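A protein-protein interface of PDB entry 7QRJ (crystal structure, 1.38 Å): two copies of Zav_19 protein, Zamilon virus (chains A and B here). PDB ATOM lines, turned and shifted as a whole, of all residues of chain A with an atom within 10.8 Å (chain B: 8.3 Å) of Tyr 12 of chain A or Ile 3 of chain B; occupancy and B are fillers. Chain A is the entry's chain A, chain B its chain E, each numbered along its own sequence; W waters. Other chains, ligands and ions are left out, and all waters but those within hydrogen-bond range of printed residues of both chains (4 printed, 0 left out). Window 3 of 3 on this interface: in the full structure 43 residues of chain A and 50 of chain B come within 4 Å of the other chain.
NE2 of His 15 of chain A lies close to O of Leu 7 of chain B.
The side-chain amide nitrogen (ND2) of Asn 10 of chain B sits at hydrogen-bond distance from the backbone carbonyl oxygen (O) of His 15 of chain A, at 2.9 Å.
The backbone NH (N) of His 15 of chain A sits at hydrogen-bond distance from the backbone carbonyl oxygen (O) of Leu 6 of chain B, at 2.8 Å.
The backbone carbonyl oxygen of Ser 5 of chain B lies within hydrogen-bond range of the side-chain amide nitrogen of Asn 10 of chain B, at 3.1 Å.
The side-chain hydroxyl of Ser 5 of chain B lies within hydrogen-bond range of the side-chain hydroxyl of Tyr 12 of chain B, at 3.3 Å.
The side-chain amide oxygen (OD1) of Asn 10 of chain B is in hydrogen-bond range of the backbone NH (N) of Tyr 12 of chain B (2.9 Å).
ND2 of Asn 10 of chain A lies within hydrogen-bond range of O of Ser 5 of chain A, 3.2 Å away.
The side-chain amide nitrogen (ND2) of Asn 10 of chain B lies within hydrogen-bond range of the backbone carbonyl oxygen (O) of Glu 8 of chain B (3.1 Å).
OD1 of Asn 10 of chain A is in hydrogen-bond range of N of Tyr 12 of chain A, at 2.9 Å.
Among the printed residues, merely in contact across the chains: Asn 13 of chain A with Pro 28 of chain B (3.4 Å), Val 14 of chain A with Leu 6 of chain B (3.4 Å), Asn 16 of chain A with Tyr 12 of chain B (3.5 Å), Tyr 12 of chain A with Leu 7 of chain B (3.6 Å), His 15 of chain A with Glu 8 of chain B (3.6 Å), Leu 6 of chain A with Leu 6 of chain B (3.7 Å), Asn 16 of chain A with Asn 10 of chain B (3.7 Å), Leu 6 of chain A with Ile 3 of chain B (3.7 Å), Ser 5 of chain A with Ile 3 of chain B (3.7 Å), Asn 13 of chain A with Leu 7 of chain B (3.8 Å), Lys 9 of chain A with Thr 22 of chain B (3.8 Å), Asn 13 of chain A with Leu 6 of chain B (3.9 Å) and Tyr 12 of chain A with Ile 3 of chain B (3.98 Å).
Of the printed residues of chain B, Leu 6 of chain A touches Ile 3 and Leu 6.
Of the printed residues of chain B, Lys 9 of chain A touches Thr 22.
Of the printed residues of chain B, Tyr 12 of chain A touches Ile 3 and Leu 7.
Of the printed residues of chain B, Asn 13 of chain A touches Leu 6, Leu 7 and Pro 28.
Printed residues of chain A within 4 Å of Ile 3 of chain B: Ser 5 (3.7 Å), Leu 6 (3.7 Å) and Tyr 12 (3.98 Å).
No residue of chain A comes within 4 Å of Ser 5 of chain B.
Of the printed residues of chain A, Asn 10 of chain B touches His 15 and Asn 16.
The nearest printed residue of chain B that does not touch Tyr 12 of chain A is Leu 6 of chain B (6.5 Å).
The nearest printed residue of chain A that does not touch Ile 3 of chain B is Ser 4 of chain A (6.2 Å).
The nearest printed residue of chain A that does not touch Tyr 12 of chain B is His 15 of chain A (5.2 Å).
Hydrophobic or aromatic side chains of chain B within 4 Å of the printed part of chain A: Ile 3, Leu 6, Leu 7 and Pro 28.
Of the 13 printed residues of chain A, 8 touch a printed residue of chain B.
Among the printed residues, no Asp or Glu carboxylate lies within 4 Å of a Lys or Arg side-chain nitrogen of the other chain.
Leu 6 of chain B touches its own counterpart, Leu 6 of chain A.
Tyr 12 of chain A touches Leu 7 of chain B, but with the chains exchanged Leu 7 of chain A does not touch Tyr 12 of chain B (14.4 Å).
Of the 16 pairs that touch across the chains among the printed residues, 1 has its exchanged pair printed and touching as well.
Water W4 lies within hydrogen-bond range of the backbone carbonyl oxygen (O) of Asn 10 of chain A (2.5 Å) and the side-chain hydroxyl (OG1) of Thr 22 of chain B (2.7 Å).
Water W1 bridges N of Asn 10 of chain B and N of Asn 16 of chain A.
Water W2 lies within hydrogen-bond range of the backbone NH (N) of Asn 10 of chain A (2.9 Å) and the side-chain hydroxyl (OG1) of Thr 22 of chain B (3.4 Å).
Water W3 lies within hydrogen-bond range of the side-chain amide nitrogen (ND2) of Asn 13 of chain A and the backbone carbonyl oxygen (O) of Pro 28 of chain B.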
ATOM      1  N   SER A   4      12.354   5.107  12.315  1.00  0.00           N
ATOM      2  CA  SER A   4      13.572   5.568  12.965  1.00  0.00           C
ATOM      3  C   SER A   4      13.214   6.231  14.288  1.00  0.00           C
ATOM      4  O   SER A   4      14.013   6.237  15.223  1.00  0.00           O
ATOM      5  CB  SER A   4      14.335   6.549  12.064  1.00  0.00           C
ATOM      6  OG  SER A   4      15.367   7.216  12.772  1.00  0.00           O
ATOM      7  N   SER A   5      12.002   6.791  14.364  1.00  0.00           N
ATOM      8  CA  SER A   5      11.577   7.431  15.604  1.00  0.00           C
ATOM      9  C   SER A   5      11.390   6.413  16.719  1.00  0.00           C
ATOM     10  O   SER A   5      11.570   6.748  17.894  1.00  0.00           O
ATOM     11  CB  SER A   5      10.321   8.282  15.387  1.00  0.00           C
ATOM     12  OG  SER A   5       9.177   7.486  15.138  1.00  0.00           O
ATOM     13  N   LEU A   6      11.051   5.168  16.370  1.00  0.00           N
ATOM     14  CA  LEU A   6      10.917   4.100  17.354  1.00  0.00           C
ATOM     15  C   LEU A   6      12.259   3.559  17.824  1.00  0.00           C
ATOM     16  O   LEU A   6      12.306   2.846  18.831  1.00  0.00           O
ATOM     17  CB  LEU A   6      10.139   2.925  16.753  1.00  0.00           C
ATOM     18  CG  LEU A   6       8.615   2.878  16.745  1.00  0.00           C
ATOM     19  CD1 LEU A   6       8.173   1.502  16.268  1.00  0.00           C
ATOM     20  CD2 LEU A   6       8.056   3.179  18.116  1.00  0.00           C
ATOM     21  N   LEU A   7      13.341   3.850  17.106  1.00  0.00           N
ATOM     22  CA  LEU A   7      14.650   3.293  17.403  1.00  0.00           C
ATOM     23  C   LEU A   7      15.457   4.167  18.354  1.00  0.00           C
ATOM     24  O   LEU A   7      16.603   3.825  18.664  1.00  0.00           O
ATOM     25  CB  LEU A   7      15.426   3.061  16.101  1.00  0.00           C
ATOM     26  CG  LEU A   7      14.693   2.154  15.102  1.00  0.00           C
ATOM     27  CD1 LEU A   7      15.567   1.869  13.892  1.00  0.00           C
ATOM     28  CD2 LEU A   7      14.243   0.853  15.756  1.00  0.00           C
ATOM     29  N   GLU A   8      14.888   5.287  18.804  1.00  0.00           N
ATOM     30  CA  GLU A   8      15.470   6.130  19.838  1.00  0.00           C
ATOM     31  C   GLU A   8      14.349   6.567  20.768  1.00  0.00           C
ATOM     32  O   GLU A   8      13.166   6.390  20.463  1.00  0.00           O
ATOM     33  CB  GLU A   8      16.197   7.346  19.241  1.00  0.00           C
ATOM     34  CG  GLU A   8      17.170   6.994  18.124  1.00  0.00           C
ATOM     35  CD  GLU A   8      17.688   8.205  17.379  1.00  0.00           C
ATOM     36  OE1 GLU A   8      16.997   9.249  17.363  1.00  0.00           O
ATOM     37  OE2 GLU A   8      18.791   8.110  16.800  1.00  0.00           O
ATOM     38  N   LYS A   9      14.723   7.150  21.908  1.00  0.00           N
ATOM     39  CA  LYS A   9      13.732   7.549  22.902  1.00  0.00           C
ATOM     40  C   LYS A   9      12.656   8.429  22.277  1.00  0.00           C
ATOM     41  O   LYS A   9      12.941   9.315  21.468  1.00  0.00           O
ATOM     42  CB  LYS A   9      14.396   8.288  24.070  1.00  0.00           C
ATOM     43  CG  LYS A   9      13.410   8.633  25.180  1.00  0.00           C
ATOM     44  CD  LYS A   9      14.087   9.204  26.413  1.00  0.00           C
ATOM     45  CE  LYS A   9      13.059   9.499  27.496  1.00  0.00           C
ATOM     46  NZ  LYS A   9      13.668  10.028  28.745  1.00  0.00           N
ATOM     47  N   ASN A  10      11.409   8.163  22.652  1.00  0.00           N
ATOM     48  CA  ASN A  10      10.264   8.908  22.157  1.00  0.00           C
ATOM     49  C   ASN A  10       9.233   8.979  23.272  1.00  0.00           C
ATOM     50  O   ASN A  10       9.402   8.381  24.340  1.00  0.00           O
ATOM     51  CB  ASN A  10       9.674   8.222  20.924  1.00  0.00           C
ATOM     52  CG  ASN A  10       9.337   6.770  21.192  1.00  0.00           C
ATOM     53  OD1 ASN A  10       8.460   6.471  22.001  1.00  0.00           O
ATOM     54  ND2 ASN A  10      10.050   5.858  20.534  1.00  0.00           N
ATOM     55  N   ILE A  11       8.134   9.686  23.014  1.00  0.00           N
ATOM     56  CA  ILE A  11       7.074   9.809  24.010  1.00  0.00           C
ATOM     57  C   ILE A  11       5.873   8.951  23.616  1.00  0.00           C
ATOM     58  O   ILE A  11       4.746   9.206  24.053  1.00  0.00           O
ATOM     59  CB  ILE A  11       6.682  11.281  24.241  1.00  0.00           C
ATOM     60  CG1 ILE A  11       6.389  11.977  22.911  1.00  0.00           C
ATOM     61  CG2 ILE A  11       7.804  12.017  24.955  1.00  0.00           C
ATOM     62  CD1 ILE A  11       5.539  13.232  23.044  1.00  0.00           C
ATOM     63  N   TYR A  12       6.110   7.906  22.816  1.00  0.00           N
ATOM     64  CA  TYR A  12       5.024   7.100  22.259  1.00  0.00           C
ATOM     65  C   TYR A  12       4.524   6.066  23.261  1.00  0.00           C
ATOM     66  O   TYR A  12       5.293   5.221  23.734  1.00  0.00           O
ATOM     67  CB  TYR A  12       5.472   6.374  20.994  1.00  0.00           C
ATOM     68  CG  TYR A  12       5.985   7.236  19.857  1.00  0.00           C
ATOM     69  CD1 TYR A  12       5.545   8.546  19.676  1.00  0.00           C
ATOM     70  CD2 TYR A  12       6.901   6.723  18.948  1.00  0.00           C
ATOM     71  CE1 TYR A  12       6.016   9.314  18.618  1.00  0.00           C
ATOM     72  CE2 TYR A  12       7.372   7.478  17.897  1.00  0.00           C
ATOM     73  CZ  TYR A  12       6.932   8.770  17.737  1.00  0.00           C
ATOM     74  OH  TYR A  12       7.415   9.510  16.683  1.00  0.00           O
ATOM     75  N   ASN A  13       3.229   6.098  23.548  1.00  0.00           N
ATOM     76  CA  ASN A  13       2.566   4.984  24.222  1.00  0.00           C
ATOM     77  C   ASN A  13       2.138   4.005  23.136  1.00  0.00           C
ATOM     78  O   ASN A  13       1.090   4.168  22.510  1.00  0.00           O
ATOM     79  CB  ASN A  13       1.404   5.483  25.073  1.00  0.00           C
ATOM     80  CG  ASN A  13       1.875   6.294  26.261  1.00  0.00           C
ATOM     81  OD1 ASN A  13       2.712   5.837  27.043  1.00  0.00           O
ATOM     82  ND2 ASN A  13       1.351   7.510  26.400  1.00  0.00           N
ATOM     83  N   VAL A  14       2.974   2.997  22.901  1.00  0.00           N
ATOM     84  CA  VAL A  14       2.777   2.040  21.817  1.00  0.00           C
ATOM     85  C   VAL A  14       1.757   0.991  22.232  1.00  0.00           C
ATOM     86  O   VAL A  14       1.745   0.526  23.378  1.00  0.00           O
ATOM     87  CB  VAL A  14       4.126   1.399  21.443  1.00  0.00           C
ATOM     88  CG1 VAL A  14       3.940   0.127  20.605  1.00  0.00           C
ATOM     89  CG2 VAL A  14       4.993   2.409  20.705  1.00  0.00           C
ATOM     90  N   HIS A  15       0.895   0.616  21.292  1.00  0.00           N
ATOM     91  CA  HIS A  15      -0.047  -0.475  21.470  1.00  0.00           C
ATOM     92  C   HIS A  15       0.315  -1.592  20.506  1.00  0.00           C
ATOM     93  O   HIS A  15       0.709  -1.332  19.365  1.00  0.00           O
ATOM     94  CB  HIS A  15      -1.474  -0.011  21.181  1.00  0.00           C
ATOM     95  CG  HIS A  15      -1.946   1.088  22.082  1.00  0.00           C
ATOM     96  ND1 HIS A  15      -3.045   0.950  22.902  1.00  0.00           N
ATOM     97  CD2 HIS A  15      -1.470   2.339  22.297  1.00  0.00           C
ATOM     98  CE1 HIS A  15      -3.226   2.067  23.584  1.00  0.00           C
ATOM     99  NE2 HIS A  15      -2.286   2.927  23.234  1.00  0.00           N
ATOM    100  N   ASN A  16       0.189  -2.832  20.972  1.00  0.00           N
ATOM    101  CA  ASN A  16       0.365  -3.987  20.102  1.00  0.00           C
ATOM    102  C   ASN A  16      -0.443  -5.163  20.634  1.00  0.00           C
ATOM    103  O   ASN A  16      -0.635  -5.309  21.845  1.00  0.00           O
ATOM    104  CB  ASN A  16       1.849  -4.357  19.863  1.00  0.00           C
ATOM    105  CG  ASN A  16       2.690  -4.388  21.147  1.00  0.00           C
ATOM    106  OD1 ASN A  16       3.896  -4.112  21.145  1.00  0.00           O
ATOM    107  ND2 ASN A  16       2.027  -4.683  22.261  1.00  0.00           N
ATOM    108  N   ILE B   3       3.210   5.037  12.159  1.00  0.00           N
ATOM    109  CA  ILE B   3       3.469   5.273  13.573  1.00  0.00           C
ATOM    110  C   ILE B   3       2.173   5.599  14.297  1.00  0.00           C
ATOM    111  O   ILE B   3       1.905   5.078  15.380  1.00  0.00           O
ATOM    112  CB  ILE B   3       4.525   6.377  13.774  1.00  0.00           C
ATOM    113  CG1 ILE B   3       5.917   5.852  13.416  1.00  0.00           C
ATOM    114  CG2 ILE B   3       4.494   6.899  15.207  1.00  0.00           C
ATOM    115  CD1 ILE B   3       6.526   4.958  14.473  1.00  0.00           C
ATOM    116  N   SER B   4       1.368   6.472  13.683  1.00  0.00           N
ATOM    117  CA  SER B   4       0.077   6.828  14.260  1.00  0.00           C
ATOM    118  C   SER B   4      -0.770   5.597  14.551  1.00  0.00           C
ATOM    119  O   SER B   4      -1.501   5.566  15.549  1.00  0.00           O
ATOM    120  CB  SER B   4      -0.669   7.776  13.319  1.00  0.00           C
ATOM    121  OG  SER B   4      -2.055   7.783  13.609  1.00  0.00           O
ATOM    122  N   SER B   5      -0.681   4.571  13.700  1.00  0.00           N
ATOM    123  CA  SER B   5      -1.422   3.341  13.942  1.00  0.00           C
ATOM    124  C   SER B   5      -0.922   2.598  15.174  1.00  0.00           C
ATOM    125  O   SER B   5      -1.694   1.853  15.782  1.00  0.00           O
ATOM    126  CB  SER B   5      -1.373   2.433  12.712  1.00  0.00           C
ATOM    127  OG  SER B   5      -0.045   2.043  12.416  1.00  0.00           O
ATOM    128  N   LEU B   6       0.343   2.793  15.555  1.00  0.00           N
ATOM    129  CA  LEU B   6       0.893   2.161  16.749  1.00  0.00           C
ATOM    130  C   LEU B   6       0.531   2.907  18.025  1.00  0.00           C
ATOM    131  O   LEU B   6       0.663   2.344  19.120  1.00  0.00           O
ATOM    132  CB  LEU B   6       2.417   2.114  16.641  1.00  0.00           C
ATOM    133  CG  LEU B   6       3.056   1.053  15.751  1.00  0.00           C
ATOM    134  CD1 LEU B   6       4.566   1.231  15.765  1.00  0.00           C
ATOM    135  CD2 LEU B   6       2.678  -0.352  16.199  1.00  0.00           C
ATOM    136  N   LEU B   7       0.102   4.164  17.913  1.00  0.00           N
ATOM    137  CA  LEU B   7      -0.243   4.961  19.082  1.00  0.00           C
ATOM    138  C   LEU B   7      -1.650   4.682  19.579  1.00  0.00           C
ATOM    139  O   LEU B   7      -2.032   5.190  20.639  1.00  0.00           O
ATOM    140  CB  LEU B   7      -0.099   6.450  18.762  1.00  0.00           C
ATOM    141  CG  LEU B   7       1.290   6.904  18.304  1.00  0.00           C
ATOM    142  CD1 LEU B   7       1.328   8.413  18.114  1.00  0.00           C
ATOM    143  CD2 LEU B   7       2.362   6.459  19.281  1.00  0.00           C
ATOM    144  N   GLU B   8      -2.429   3.903  18.836  1.00  0.00           N
ATOM    145  CA  GLU B   8      -3.755   3.482  19.251  1.00  0.00           C
ATOM    146  C   GLU B   8      -3.884   1.988  18.998  1.00  0.00           C
ATOM    147  O   GLU B   8      -3.062   1.382  18.305  1.00  0.00           O
ATOM    148  CB  GLU B   8      -4.859   4.240  18.498  1.00  0.00           C
ATOM    149  CG  GLU B   8      -4.430   5.580  17.921  1.00  0.00           C
ATOM    150  CD  GLU B   8      -5.585   6.344  17.305  1.00  0.00           C
ATOM    151  OE1 GLU B   8      -6.587   5.703  16.918  1.00  0.00           O
ATOM    152  OE2 GLU B   8      -5.490   7.586  17.204  1.00  0.00           O
ATOM    153  N   ASN B  10      -4.441  -1.639  17.822  1.00  0.00           N
ATOM    154  CA  ASN B  10      -4.280  -2.241  16.508  1.00  0.00           C
ATOM    155  C   ASN B  10      -4.255  -3.755  16.681  1.00  0.00           C
ATOM    156  O   ASN B  10      -4.301  -4.268  17.803  1.00  0.00           O
ATOM    157  CB  ASN B  10      -2.996  -1.732  15.857  1.00  0.00           C
ATOM    158  CG  ASN B  10      -1.787  -1.956  16.734  1.00  0.00           C
ATOM    159  OD1 ASN B  10      -1.405  -3.093  16.998  1.00  0.00           O
ATOM    160  ND2 ASN B  10      -1.168  -0.870  17.184  1.00  0.00           N
ATOM    161  N   TYR B  12      -1.658  -5.554  15.544  1.00  0.00           N
ATOM    162  CA  TYR B  12      -0.280  -5.863  15.166  1.00  0.00           C
ATOM    163  C   TYR B  12       0.403  -6.758  16.192  1.00  0.00           C
ATOM    164  O   TYR B  12       0.520  -6.395  17.368  1.00  0.00           O
ATOM    165  CB  TYR B  12       0.549  -4.592  15.012  1.00  0.00           C
ATOM    166  CG  TYR B  12       0.034  -3.587  14.016  1.00  0.00           C
ATOM    167  CD1 TYR B  12      -0.613  -3.991  12.858  1.00  0.00           C
ATOM    168  CD2 TYR B  12       0.227  -2.231  14.221  1.00  0.00           C
ATOM    169  CE1 TYR B  12      -1.072  -3.062  11.937  1.00  0.00           C
ATOM    170  CE2 TYR B  12      -0.225  -1.296  13.313  1.00  0.00           C
ATOM    171  CZ  TYR B  12      -0.874  -1.717  12.173  1.00  0.00           C
ATOM    172  OH  TYR B  12      -1.324  -0.778  11.272  1.00  0.00           O
ATOM    173  N   THR B  20      12.543  -1.146  25.040  1.00  0.00           N
ATOM    174  CA  THR B  20      13.038  -0.274  26.105  1.00  0.00           C
ATOM    175  C   THR B  20      11.926   0.668  26.564  1.00  0.00           C
ATOM    176  O   THR B  20      11.380   1.431  25.762  1.00  0.00           O
ATOM    177  CB  THR B  20      14.249   0.524  25.625  1.00  0.00           C
ATOM    178  OG1 THR B  20      15.320  -0.376  25.312  1.00  0.00           O
ATOM    179  CG2 THR B  20      14.718   1.511  26.687  1.00  0.00           C
ATOM    180  N   LEU B  21      11.596   0.603  27.853  1.00  0.00           N
ATOM    181  CA  LEU B  21      10.492   1.343  28.453  1.00  0.00           C
ATOM    182  C   LEU B  21      11.033   2.551  29.205  1.00  0.00           C
ATOM    183  O   LEU B  21      11.850   2.393  30.114  1.00  0.00           O
ATOM    184  CB  LEU B  21       9.752   0.443  29.438  1.00  0.00           C
ATOM    185  CG  LEU B  21       9.129  -0.818  28.844  1.00  0.00           C
ATOM    186  CD1 LEU B  21       9.041  -1.909  29.887  1.00  0.00           C
ATOM    187  CD2 LEU B  21       7.754  -0.495  28.263  1.00  0.00           C
ATOM    188  N   THR B  22      10.546   3.747  28.866  1.00  0.00           N
ATOM    189  CA  THR B  22      10.994   4.961  29.553  1.00  0.00           C
ATOM    190  C   THR B  22      10.723   4.876  31.052  1.00  0.00           C
ATOM    191  O   THR B  22       9.641   4.463  31.479  1.00  0.00           O
ATOM    192  CB  THR B  22      10.269   6.182  28.989  1.00  0.00           C
ATOM    193  OG1 THR B  22      10.507   6.261  27.582  1.00  0.00           O
ATOM    194  CG2 THR B  22      10.748   7.463  29.671  1.00  0.00           C
ATOM    195  N   PRO B  28       1.702   5.506  32.398  1.00  0.00           N
ATOM    196  CA  PRO B  28       1.405   6.616  31.467  1.00  0.00           C
ATOM    197  C   PRO B  28       0.005   6.567  30.885  1.00  0.00           C
ATOM    198  O   PRO B  28      -0.506   7.617  30.486  1.00  0.00           O
ATOM    199  CB  PRO B  28       2.445   6.410  30.358  1.00  0.00           C
ATOM    200  CG  PRO B  28       3.592   5.769  31.041  1.00  0.00           C
ATOM    201  CD  PRO B  28       2.990   4.842  32.075  1.00  0.00           C
ATOM    202  N   THR B  29      -0.621   5.390  30.805  1.00  0.00           N
ATOM    203  CA  THR B  29      -1.969   5.278  30.264  1.00  0.00           C
ATOM    204  C   THR B  29      -3.030   5.069  31.328  1.00  0.00           C
ATOM    205  O   THR B  29      -4.204   5.358  31.069  1.00  0.00           O
ATOM    206  CB  THR B  29      -2.071   4.079  29.313  1.00  0.00           C
ATOM    207  OG1 THR B  29      -1.937   2.873  30.078  1.00  0.00           O
ATOM    208  CG2 THR B  29      -0.982   4.142  28.241  1.00  0.00           C
ATOM    209  N   VAL B  35       2.379  -2.126  30.128  1.00  0.00           N
ATOM    210  CA  VAL B  35       3.694  -2.380  30.700  1.00  0.00           C
ATOM    211  C   VAL B  35       4.468  -1.065  30.719  1.00  0.00           C
ATOM    212  O   VAL B  35       4.470  -0.317  29.731  1.00  0.00           O
ATOM    213  CB  VAL B  35       4.429  -3.456  29.876  1.00  0.00           C
ATOM    214  CG1 VAL B  35       5.788  -3.741  30.450  1.00  0.00           C
ATOM    215  CG2 VAL B  35       3.607  -4.739  29.843  1.00  0.00           C
HETATM  216  O   HOH W   1      -2.807  -2.808  19.898  1.00  0.00           O
HETATM  217  O   HOH W   2      10.749   5.786  24.194  1.00  0.00           O
HETATM  218  O   HOH W   3       1.624   9.503  28.625  1.00  0.00           O
HETATM  219  O   HOH W   4       9.213   8.536  26.877  1.00  0.00           O
